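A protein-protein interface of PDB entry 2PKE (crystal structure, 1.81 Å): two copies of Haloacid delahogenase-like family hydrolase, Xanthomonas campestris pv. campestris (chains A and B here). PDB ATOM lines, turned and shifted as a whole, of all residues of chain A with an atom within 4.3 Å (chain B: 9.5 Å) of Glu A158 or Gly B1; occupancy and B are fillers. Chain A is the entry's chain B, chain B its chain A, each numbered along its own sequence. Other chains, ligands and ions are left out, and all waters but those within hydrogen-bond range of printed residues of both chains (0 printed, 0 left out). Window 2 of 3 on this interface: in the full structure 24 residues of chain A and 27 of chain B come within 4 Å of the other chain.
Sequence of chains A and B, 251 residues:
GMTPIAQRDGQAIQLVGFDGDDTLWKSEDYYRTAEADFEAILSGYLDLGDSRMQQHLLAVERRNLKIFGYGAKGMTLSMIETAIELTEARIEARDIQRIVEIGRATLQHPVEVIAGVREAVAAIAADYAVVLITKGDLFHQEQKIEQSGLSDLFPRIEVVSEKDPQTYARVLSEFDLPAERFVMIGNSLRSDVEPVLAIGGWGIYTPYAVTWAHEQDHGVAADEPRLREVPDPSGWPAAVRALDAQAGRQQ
The side-chain carboxylate (OE1) of Glu A158 lies within hydrogen-bond range of the backbone NH (N) of Gly B1 (3.1 Å).
N of Gly B1 lies within hydrogen-bond range of OE1 of Glu A174, 3.2 Å away.
The backbone carbonyl oxygen (O) of Leu A132 sits at hydrogen-bond distance from the backbone NH (N) of Glu A158, at 2.8 Å.
The backbone carbonyl oxygen of Glu A158 lies within hydrogen-bond range of the backbone NH of Thr A134, at 2.9 Å.
The backbone NH of Val A160 lies within hydrogen-bond range of the backbone carbonyl oxygen of Thr A134.
Among the printed residues, merely in contact across the chains: Val A159 with Leu B138, Val A160 with Leu B138 and Glu A174 with Thr B3.
Of chain B, only Gly B1 comes within 4 Å of Glu A158.
Of chain A, only Glu A158 and Glu A174 come within 4 Å of Gly B1.
Val A159 touches one residue of chain B.
Of the printed residues of chain B, Glu A174 touches Gly B1 and Thr B3.
Of the printed residues of chain A, Thr B3 touches Glu A174 (3.3 Å).
Printed residues of chain B within 4 Å of Val A160: Leu B138 (3.7 Å).
Arg B156 touches none of the printed residues of chain A.
The nearest printed residue of chain A that does not touch Gly B1 is Ile A157 (6.0 Å).
Among the printed residues, 5 pairs touch across the chains.
6 positions are printed for both chains.
Of the 5 pairs that touch across the chains among the printed residues, none has its exchanged pair printed and touching as well.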
ATOM      1  N   VAL A 131      16.469  -9.214  18.268  1.00  0.00           N
ATOM      2  CA  VAL A 131      17.080  -8.086  17.654  1.00  0.00           C
ATOM      3  C   VAL A 131      16.025  -6.989  17.488  1.00  0.00           C
ATOM      4  O   VAL A 131      14.868  -7.257  17.168  1.00  0.00           O
ATOM      5  CB  VAL A 131      17.697  -8.506  16.300  1.00  0.00           C
ATOM      6  CG1 VAL A 131      16.605  -9.008  15.333  1.00  0.00           C
ATOM      7  CG2 VAL A 131      18.539  -7.391  15.731  1.00  0.00           C
ATOM      8  N   LEU A 132      16.425  -5.754  17.739  1.00  0.00           N
ATOM      9  CA  LEU A 132      15.568  -4.625  17.443  1.00  0.00           C
ATOM     10  C   LEU A 132      15.978  -4.108  16.059  1.00  0.00           C
ATOM     11  O   LEU A 132      17.155  -3.882  15.806  1.00  0.00           O
ATOM     12  CB  LEU A 132      15.730  -3.571  18.529  1.00  0.00           C
ATOM     13  CG  LEU A 132      14.735  -2.448  18.766  1.00  0.00           C
ATOM     14  CD1 LEU A 132      15.031  -1.853  20.206  1.00  0.00           C
ATOM     15  CD2 LEU A 132      14.764  -1.372  17.699  1.00  0.00           C
ATOM     16  N   ILE A 133      15.020  -3.997  15.158  1.00  0.00           N
ATOM     17  CA  ILE A 133      15.260  -3.464  13.805  1.00  0.00           C
ATOM     18  C   ILE A 133      14.331  -2.279  13.613  1.00  0.00           C
ATOM     19  O   ILE A 133      13.118  -2.443  13.522  1.00  0.00           O
ATOM     20  CB  ILE A 133      15.000  -4.486  12.735  1.00  0.00           C
ATOM     21  CG1 ILE A 133      15.819  -5.747  13.068  1.00  0.00           C
ATOM     22  CG2 ILE A 133      15.298  -3.871  11.337  1.00  0.00           C
ATOM     23  CD1 ILE A 133      15.553  -6.974  12.170  1.00  0.00           C
ATOM     24  N   THR A 134      14.909  -1.092  13.592  1.00  0.00           N
ATOM     25  CA  THR A 134      14.114   0.123  13.537  1.00  0.00           C
ATOM     26  C   THR A 134      14.622   0.975  12.390  1.00  0.00           C
ATOM     27  O   THR A 134      15.815   1.113  12.177  1.00  0.00           O
ATOM     28  CB  THR A 134      14.172   0.881  14.905  1.00  0.00           C
ATOM     29  OG1 THR A 134      13.271   1.980  14.899  1.00  0.00           O
ATOM     30  CG2 THR A 134      15.589   1.381  15.235  1.00  0.00           C
ATOM     31  N   ILE A 157      21.000  -4.401  18.160  1.00  0.00           N
ATOM     32  CA  ILE A 157      20.125  -3.320  17.750  1.00  0.00           C
ATOM     33  C   ILE A 157      20.575  -2.794  16.393  1.00  0.00           C
ATOM     34  O   ILE A 157      21.758  -2.519  16.208  1.00  0.00           O
ATOM     35  CB  ILE A 157      20.167  -2.187  18.778  1.00  0.00           C
ATOM     36  CG1 ILE A 157      19.615  -2.731  20.120  1.00  0.00           C
ATOM     37  CG2 ILE A 157      19.327  -0.962  18.286  1.00  0.00           C
ATOM     38  CD1 ILE A 157      19.459  -1.666  21.197  1.00  0.00           C
ATOM     39  N   GLU A 158      19.633  -2.694  15.461  1.00  0.00           N
ATOM     40  CA  GLU A 158      19.879  -2.261  14.097  1.00  0.00           C
ATOM     41  C   GLU A 158      19.012  -1.067  13.752  1.00  0.00           C
ATOM     42  O   GLU A 158      17.795  -1.166  13.735  1.00  0.00           O
ATOM     43  CB  GLU A 158      19.523  -3.414  13.135  1.00  0.00           C
ATOM     44  CG  GLU A 158      20.469  -4.624  13.145  1.00  0.00           C
ATOM     45  CD  GLU A 158      21.967  -4.244  13.004  1.00  0.00           C
ATOM     46  OE1 GLU A 158      22.284  -3.205  12.377  1.00  0.00           O
ATOM     47  OE2 GLU A 158      22.813  -4.987  13.546  1.00  0.00           O
ATOM     48  N   VAL A 159      19.608   0.076  13.434  1.00  0.00           N
ATOM     49  CA  VAL A 159      18.837   1.188  12.903  1.00  0.00           C
ATOM     50  C   VAL A 159      19.174   1.182  11.406  1.00  0.00           C
ATOM     51  O   VAL A 159      20.355   1.152  11.022  1.00  0.00           O
ATOM     52  CB  VAL A 159      19.229   2.568  13.526  1.00  0.00           C
ATOM     53  CG1 VAL A 159      18.438   3.702  12.885  1.00  0.00           C
ATOM     54  CG2 VAL A 159      19.060   2.562  15.080  1.00  0.00           C
ATOM     55  N   VAL A 160      18.153   1.257  10.573  1.00  0.00           N
ATOM     56  CA  VAL A 160      18.326   1.139   9.122  1.00  0.00           C
ATOM     57  C   VAL A 160      17.649   2.305   8.455  1.00  0.00           C
ATOM     58  O   VAL A 160      16.794   2.953   9.062  1.00  0.00           O
ATOM     59  CB  VAL A 160      17.753  -0.206   8.606  1.00  0.00           C
ATOM     60  CG1 VAL A 160      18.475  -1.334   9.278  1.00  0.00           C
ATOM     61  CG2 VAL A 160      16.310  -0.316   8.933  1.00  0.00           C
ATOM     62  N   VAL A 171      20.677  -7.919   7.333  1.00  0.00           N
ATOM     63  CA  VAL A 171      20.679  -8.110   8.780  1.00  0.00           C
ATOM     64  C   VAL A 171      20.822  -9.578   9.112  1.00  0.00           C
ATOM     65  O   VAL A 171      21.663  -9.925   9.918  1.00  0.00           O
ATOM     66  CB  VAL A 171      19.427  -7.515   9.484  1.00  0.00           C
ATOM     67  CG1 VAL A 171      19.442  -7.832  11.012  1.00  0.00           C
ATOM     68  CG2 VAL A 171      19.328  -5.989   9.245  1.00  0.00           C
ATOM     69  N   GLU A 174      24.252 -11.178   8.594  1.00  0.00           N
ATOM     70  CA  GLU A 174      25.185 -10.910   9.697  1.00  0.00           C
ATOM     71  C   GLU A 174      24.983 -11.859  10.874  1.00  0.00           C
ATOM     72  O   GLU A 174      25.911 -12.072  11.639  1.00  0.00           O
ATOM     73  CB  GLU A 174      25.018  -9.490  10.178  1.00  0.00           C
ATOM     74  CG  GLU A 174      25.345  -8.465   9.119  1.00  0.00           C
ATOM     75  CD  GLU A 174      24.720  -7.118   9.386  1.00  0.00           C
ATOM     76  OE1 GLU A 174      24.178  -6.922  10.499  1.00  0.00           O
ATOM     77  OE2 GLU A 174      24.793  -6.260   8.480  1.00  0.00           O
ATOM     78  N   GLY B   1      25.113  -4.083  11.513  1.00  0.00           N
ATOM     79  CA  GLY B   1      26.019  -4.615  12.564  1.00  0.00           C
ATOM     80  C   GLY B   1      27.251  -5.256  11.939  1.00  0.00           C
ATOM     81  O   GLY B   1      27.151  -6.052  11.004  1.00  0.00           O
ATOM     82  N   MET B   2      28.425  -4.898  12.447  1.00  0.00           N
ATOM     83  CA  MET B   2      29.676  -5.497  11.961  1.00  0.00           C
ATOM     84  C   MET B   2      29.765  -6.989  12.358  1.00  0.00           C
ATOM     85  O   MET B   2      29.204  -7.403  13.382  1.00  0.00           O
ATOM     86  CB  MET B   2      30.876  -4.712  12.507  1.00  0.00           C
ATOM     87  CG  MET B   2      30.874  -3.206  12.165  1.00  0.00           C
ATOM     88  SD  MET B   2      30.775  -2.877  10.203  1.00  0.00           S
ATOM     89  CE  MET B   2      28.887  -2.294   9.989  1.00  0.00           C
ATOM     90  N   THR B   3      30.443  -7.793  11.537  1.00  0.00           N
ATOM     91  CA  THR B   3      30.631  -9.217  11.842  1.00  0.00           C
ATOM     92  C   THR B   3      32.128  -9.551  11.876  1.00  0.00           C
ATOM     93  O   THR B   3      32.931  -8.891  11.205  1.00  0.00           O
ATOM     94  CB  THR B   3      29.879 -10.142  10.843  1.00  0.00           C
ATOM     95  OG1 THR B   3      30.221  -9.791   9.494  1.00  0.00           O
ATOM     96  CG2 THR B   3      28.361 -10.026  11.025  1.00  0.00           C
ATOM     97  N   PRO B   4      32.509 -10.564  12.674  1.00  0.00           N
ATOM     98  CA  PRO B   4      33.932 -10.787  12.913  1.00  0.00           C
ATOM     99  C   PRO B   4      34.781 -10.917  11.644  1.00  0.00           C
ATOM    100  O   PRO B   4      34.421 -11.641  10.737  1.00  0.00           O
ATOM    101  CB  PRO B   4      33.948 -12.073  13.747  1.00  0.00           C
ATOM    102  CG  PRO B   4      32.646 -12.065  14.450  1.00  0.00           C
ATOM    103  CD  PRO B   4      31.688 -11.541  13.421  1.00  0.00           C
ATOM    104  N   VAL B 131      36.813  -0.717   6.455  1.00  0.00           N
ATOM    105  CA  VAL B 131      35.485  -0.328   6.903  1.00  0.00           C
ATOM    106  C   VAL B 131      35.384   1.203   6.791  1.00  0.00           C
ATOM    107  O   VAL B 131      36.328   1.923   7.059  1.00  0.00           O
ATOM    108  CB  VAL B 131      35.164  -0.833   8.380  1.00  0.00           C
ATOM    109  CG1 VAL B 131      36.309  -0.474   9.393  1.00  0.00           C
ATOM    110  CG2 VAL B 131      33.759  -0.321   8.848  1.00  0.00           C
ATOM    111  N   LEU B 138      22.607   8.834   8.956  1.00  0.00           N
ATOM    112  CA  LEU B 138      22.723   7.542   8.319  1.00  0.00           C
ATOM    113  C   LEU B 138      22.307   7.554   6.866  1.00  0.00           C
ATOM    114  O   LEU B 138      22.981   7.001   6.021  1.00  0.00           O
ATOM    115  CB  LEU B 138      21.814   6.538   9.006  1.00  0.00           C
ATOM    116  CG  LEU B 138      21.765   5.112   8.476  1.00  0.00           C
ATOM    117  CD1 LEU B 138      23.071   4.361   8.728  1.00  0.00           C
ATOM    118  CD2 LEU B 138      20.636   4.434   9.144  1.00  0.00           C
ATOM    119  N   GLU B 142      24.934   7.144   3.834  1.00  0.00           N
ATOM    120  CA  GLU B 142      24.720   6.021   2.919  1.00  0.00           C
ATOM    121  C   GLU B 142      24.622   6.480   1.463  1.00  0.00           C
ATOM    122  O   GLU B 142      25.185   5.868   0.560  1.00  0.00           O
ATOM    123  CB  GLU B 142      23.473   5.272   3.303  1.00  0.00           C
ATOM    124  CG  GLU B 142      23.693   4.293   4.428  1.00  0.00           C
ATOM    125  CD  GLU B 142      22.401   3.572   4.759  1.00  0.00           C
ATOM    126  OE1 GLU B 142      21.344   3.982   4.241  1.00  0.00           O
ATOM    127  OE2 GLU B 142      22.444   2.620   5.547  1.00  0.00           O
ATOM    128  N   PRO B 155      31.801  -2.435   1.380  1.00  0.00           N
ATOM    129  CA  PRO B 155      30.628  -3.206   1.772  1.00  0.00           C
ATOM    130  C   PRO B 155      30.341  -2.984   3.304  1.00  0.00           C
ATOM    131  O   PRO B 155      29.195  -2.648   3.701  1.00  0.00           O
ATOM    132  CB  PRO B 155      31.027  -4.657   1.422  1.00  0.00           C
ATOM    133  CG  PRO B 155      32.552  -4.691   1.503  1.00  0.00           C
ATOM    134  CD  PRO B 155      32.989  -3.280   1.133  1.00  0.00           C
ATOM    135  N   ARG B 156      31.394  -3.090   4.127  1.00  0.00           N
ATOM    136  CA  ARG B 156      31.296  -2.724   5.549  1.00  0.00           C
ATOM    137  C   ARG B 156      31.185  -1.199   5.761  1.00  0.00           C
ATOM    138  O   ARG B 156      32.171  -0.445   5.523  1.00  0.00           O
ATOM    139  CB  ARG B 156      32.531  -3.214   6.315  1.00  0.00           C
ATOM    140  CG  ARG B 156      32.853  -4.671   6.169  1.00  0.00           C
ATOM    141  CD  ARG B 156      34.170  -4.977   6.837  1.00  0.00           C
ATOM    142  NE  ARG B 156      34.248  -6.401   7.117  1.00  0.00           N
ATOM    143  CZ  ARG B 156      34.738  -7.313   6.286  1.00  0.00           C
ATOM    144  NH1 ARG B 156      35.240  -6.963   5.103  1.00  0.00           N
ATOM    145  NH2 ARG B 156      34.733  -8.594   6.647  1.00  0.00           N
ATOM    146  N   ILE B 157      30.013  -0.754   6.230  1.00  0.00           N
ATOM    147  CA  ILE B 157      29.760   0.683   6.522  1.00  0.00           C
ATOM    148  C   ILE B 157      29.061   0.915   7.867  1.00  0.00           C
ATOM    149  O   ILE B 157      28.035   0.291   8.148  1.00  0.00           O
ATOM    150  CB  ILE B 157      28.927   1.270   5.427  1.00  0.00           C
ATOM    151  CG1 ILE B 157      28.505   2.695   5.789  1.00  0.00           C
ATOM    152  CG2 ILE B 157      27.827   0.274   5.074  1.00  0.00           C
ATOM    153  CD1 ILE B 157      27.078   3.024   5.470  1.00  0.00           C
ATOM    154  N   GLU B 158      29.614   1.826   8.666  1.00  0.00           N
ATOM    155  CA  GLU B 158      29.222   1.995  10.064  1.00  0.00           C
ATOM    156  C   GLU B 158      29.017   3.462  10.340  1.00  0.00           C
ATOM    157  O   GLU B 158      29.978   4.258  10.416  1.00  0.00           O
ATOM    158  CB  GLU B 158      30.299   1.410  10.966  1.00  0.00           C
ATOM    159  CG  GLU B 158      30.029   1.505  12.444  1.00  0.00           C
ATOM    160  CD  GLU B 158      28.910   0.608  12.933  1.00  0.00           C
ATOM    161  OE1 GLU B 158      28.519  -0.333  12.196  1.00  0.00           O
ATOM    162  OE2 GLU B 158      28.450   0.847  14.087  1.00  0.00           O
ATOM    163  N   VAL B 159      27.759   3.835  10.504  1.00  0.00           N
ATOM    164  CA  VAL B 159      27.399   5.178  10.874  1.00  0.00           C
ATOM    165  C   VAL B 159      27.055   5.208  12.367  1.00  0.00           C
ATOM    166  O   VAL B 159      26.227   4.463  12.842  1.00  0.00           O
ATOM    167  CB  VAL B 159      26.176   5.722  10.030  1.00  0.00           C
ATOM    168  CG1 VAL B 159      25.911   7.176  10.385  1.00  0.00           C
ATOM    169  CG2 VAL B 159      26.460   5.610   8.486  1.00  0.00           C
ATOM    170  N   ARG B 170      33.082  -0.386  20.717  1.00  0.00           N
ATOM    171  CA  ARG B 170      31.898  -1.137  20.393  1.00  0.00           C
ATOM    172  C   ARG B 170      31.996  -1.681  18.958  1.00  0.00           C
ATOM    173  O   ARG B 170      31.754  -2.880  18.714  1.00  0.00           O
ATOM    174  CB  ARG B 170      30.676  -0.260  20.582  1.00  0.00           C
ATOM    175  CG  ARG B 170      29.430  -0.908  20.021  1.00  0.00           C
ATOM    176  CD  ARG B 170      28.211  -0.024  20.065  1.00  0.00           C
ATOM    177  NE  ARG B 170      28.140   1.118  19.140  1.00  0.00           N
ATOM    178  CZ  ARG B 170      28.204   1.099  17.797  1.00  0.00           C
ATOM    179  NH1 ARG B 170      28.439  -0.018  17.108  1.00  0.00           N
ATOM    180  NH2 ARG B 170      28.047   2.250  17.133  1.00  0.00           N
ATOM    181  N   VAL B 171      32.431  -0.826  18.029  1.00  0.00           N
ATOM    182  CA  VAL B 171      32.559  -1.225  16.625  1.00  0.00           C
ATOM    183  C   VAL B 171      33.546  -2.380  16.549  1.00  0.00           C
ATOM    184  O   VAL B 171      33.239  -3.442  15.967  1.00  0.00           O
ATOM    185  CB  VAL B 171      33.001  -0.060  15.724  1.00  0.00           C
ATOM    186  CG1 VAL B 171      33.315  -0.535  14.310  1.00  0.00           C
ATOM    187  CG2 VAL B 171      31.935   1.022  15.697  1.00  0.00           C
ATOM    188  N   SER B 173      34.424  -4.458  18.882  1.00  0.00           N
ATOM    189  CA  SER B 173      33.947  -5.661  19.569  1.00  0.00           C
ATOM    190  C   SER B 173      33.096  -6.514  18.626  1.00  0.00           C
ATOM    191  O   SER B 173      33.121  -7.750  18.670  1.00  0.00           O
ATOM    192  CB  SER B 173      33.133  -5.312  20.826  1.00  0.00           C
ATOM    193  OG  SER B 173      31.826  -4.905  20.462  1.00  0.00           O
ATOM    194  N   GLU B 174      32.365  -5.847  17.748  1.00  0.00           N
ATOM    195  CA  GLU B 174      31.567  -6.551  16.757  1.00  0.00           C
ATOM    196  C   GLU B 174      32.382  -7.228  15.678  1.00  0.00           C
ATOM    197  O   GLU B 174      31.970  -8.247  15.177  1.00  0.00           O
ATOM    198  CB  GLU B 174      30.625  -5.589  16.109  1.00  0.00           C
ATOM    199  CG  GLU B 174      29.585  -5.120  17.083  1.00  0.00           C
ATOM    200  CD  GLU B 174      28.689  -4.085  16.491  1.00  0.00           C
ATOM    201  OE1 GLU B 174      28.708  -3.912  15.248  1.00  0.00           O
ATOM    202  OE2 GLU B 174      27.982  -3.441  17.287  1.00  0.00           O
ATOM    203  N   PHE B 175      33.516  -6.646  15.308  1.00  0.00           N
ATOM    204  CA  PHE B 175      34.470  -7.290  14.421  1.00  0.00           C
ATOM    205  C   PHE B 175      35.299  -8.316  15.158  1.00  0.00           C
ATOM    206  O   PHE B 175      36.059  -9.053  14.520  1.00  0.00           O
ATOM    207  CB  PHE B 175      35.460  -6.285  13.845  1.00  0.00           C
ATOM    208  CG  PHE B 175      34.888  -5.394  12.787  1.00  0.00           C
ATOM    209  CD1 PHE B 175      34.462  -5.929  11.574  1.00  0.00           C
ATOM    210  CD2 PHE B 175      34.838  -4.021  12.976  1.00  0.00           C
ATOM    211  CE1 PHE B 175      33.951  -5.111  10.586  1.00  0.00           C
ATOM    212  CE2 PHE B 175      34.329  -3.194  11.994  1.00  0.00           C
ATOM    213  CZ  PHE B 175      33.877  -3.750  10.798  1.00  0.00           C
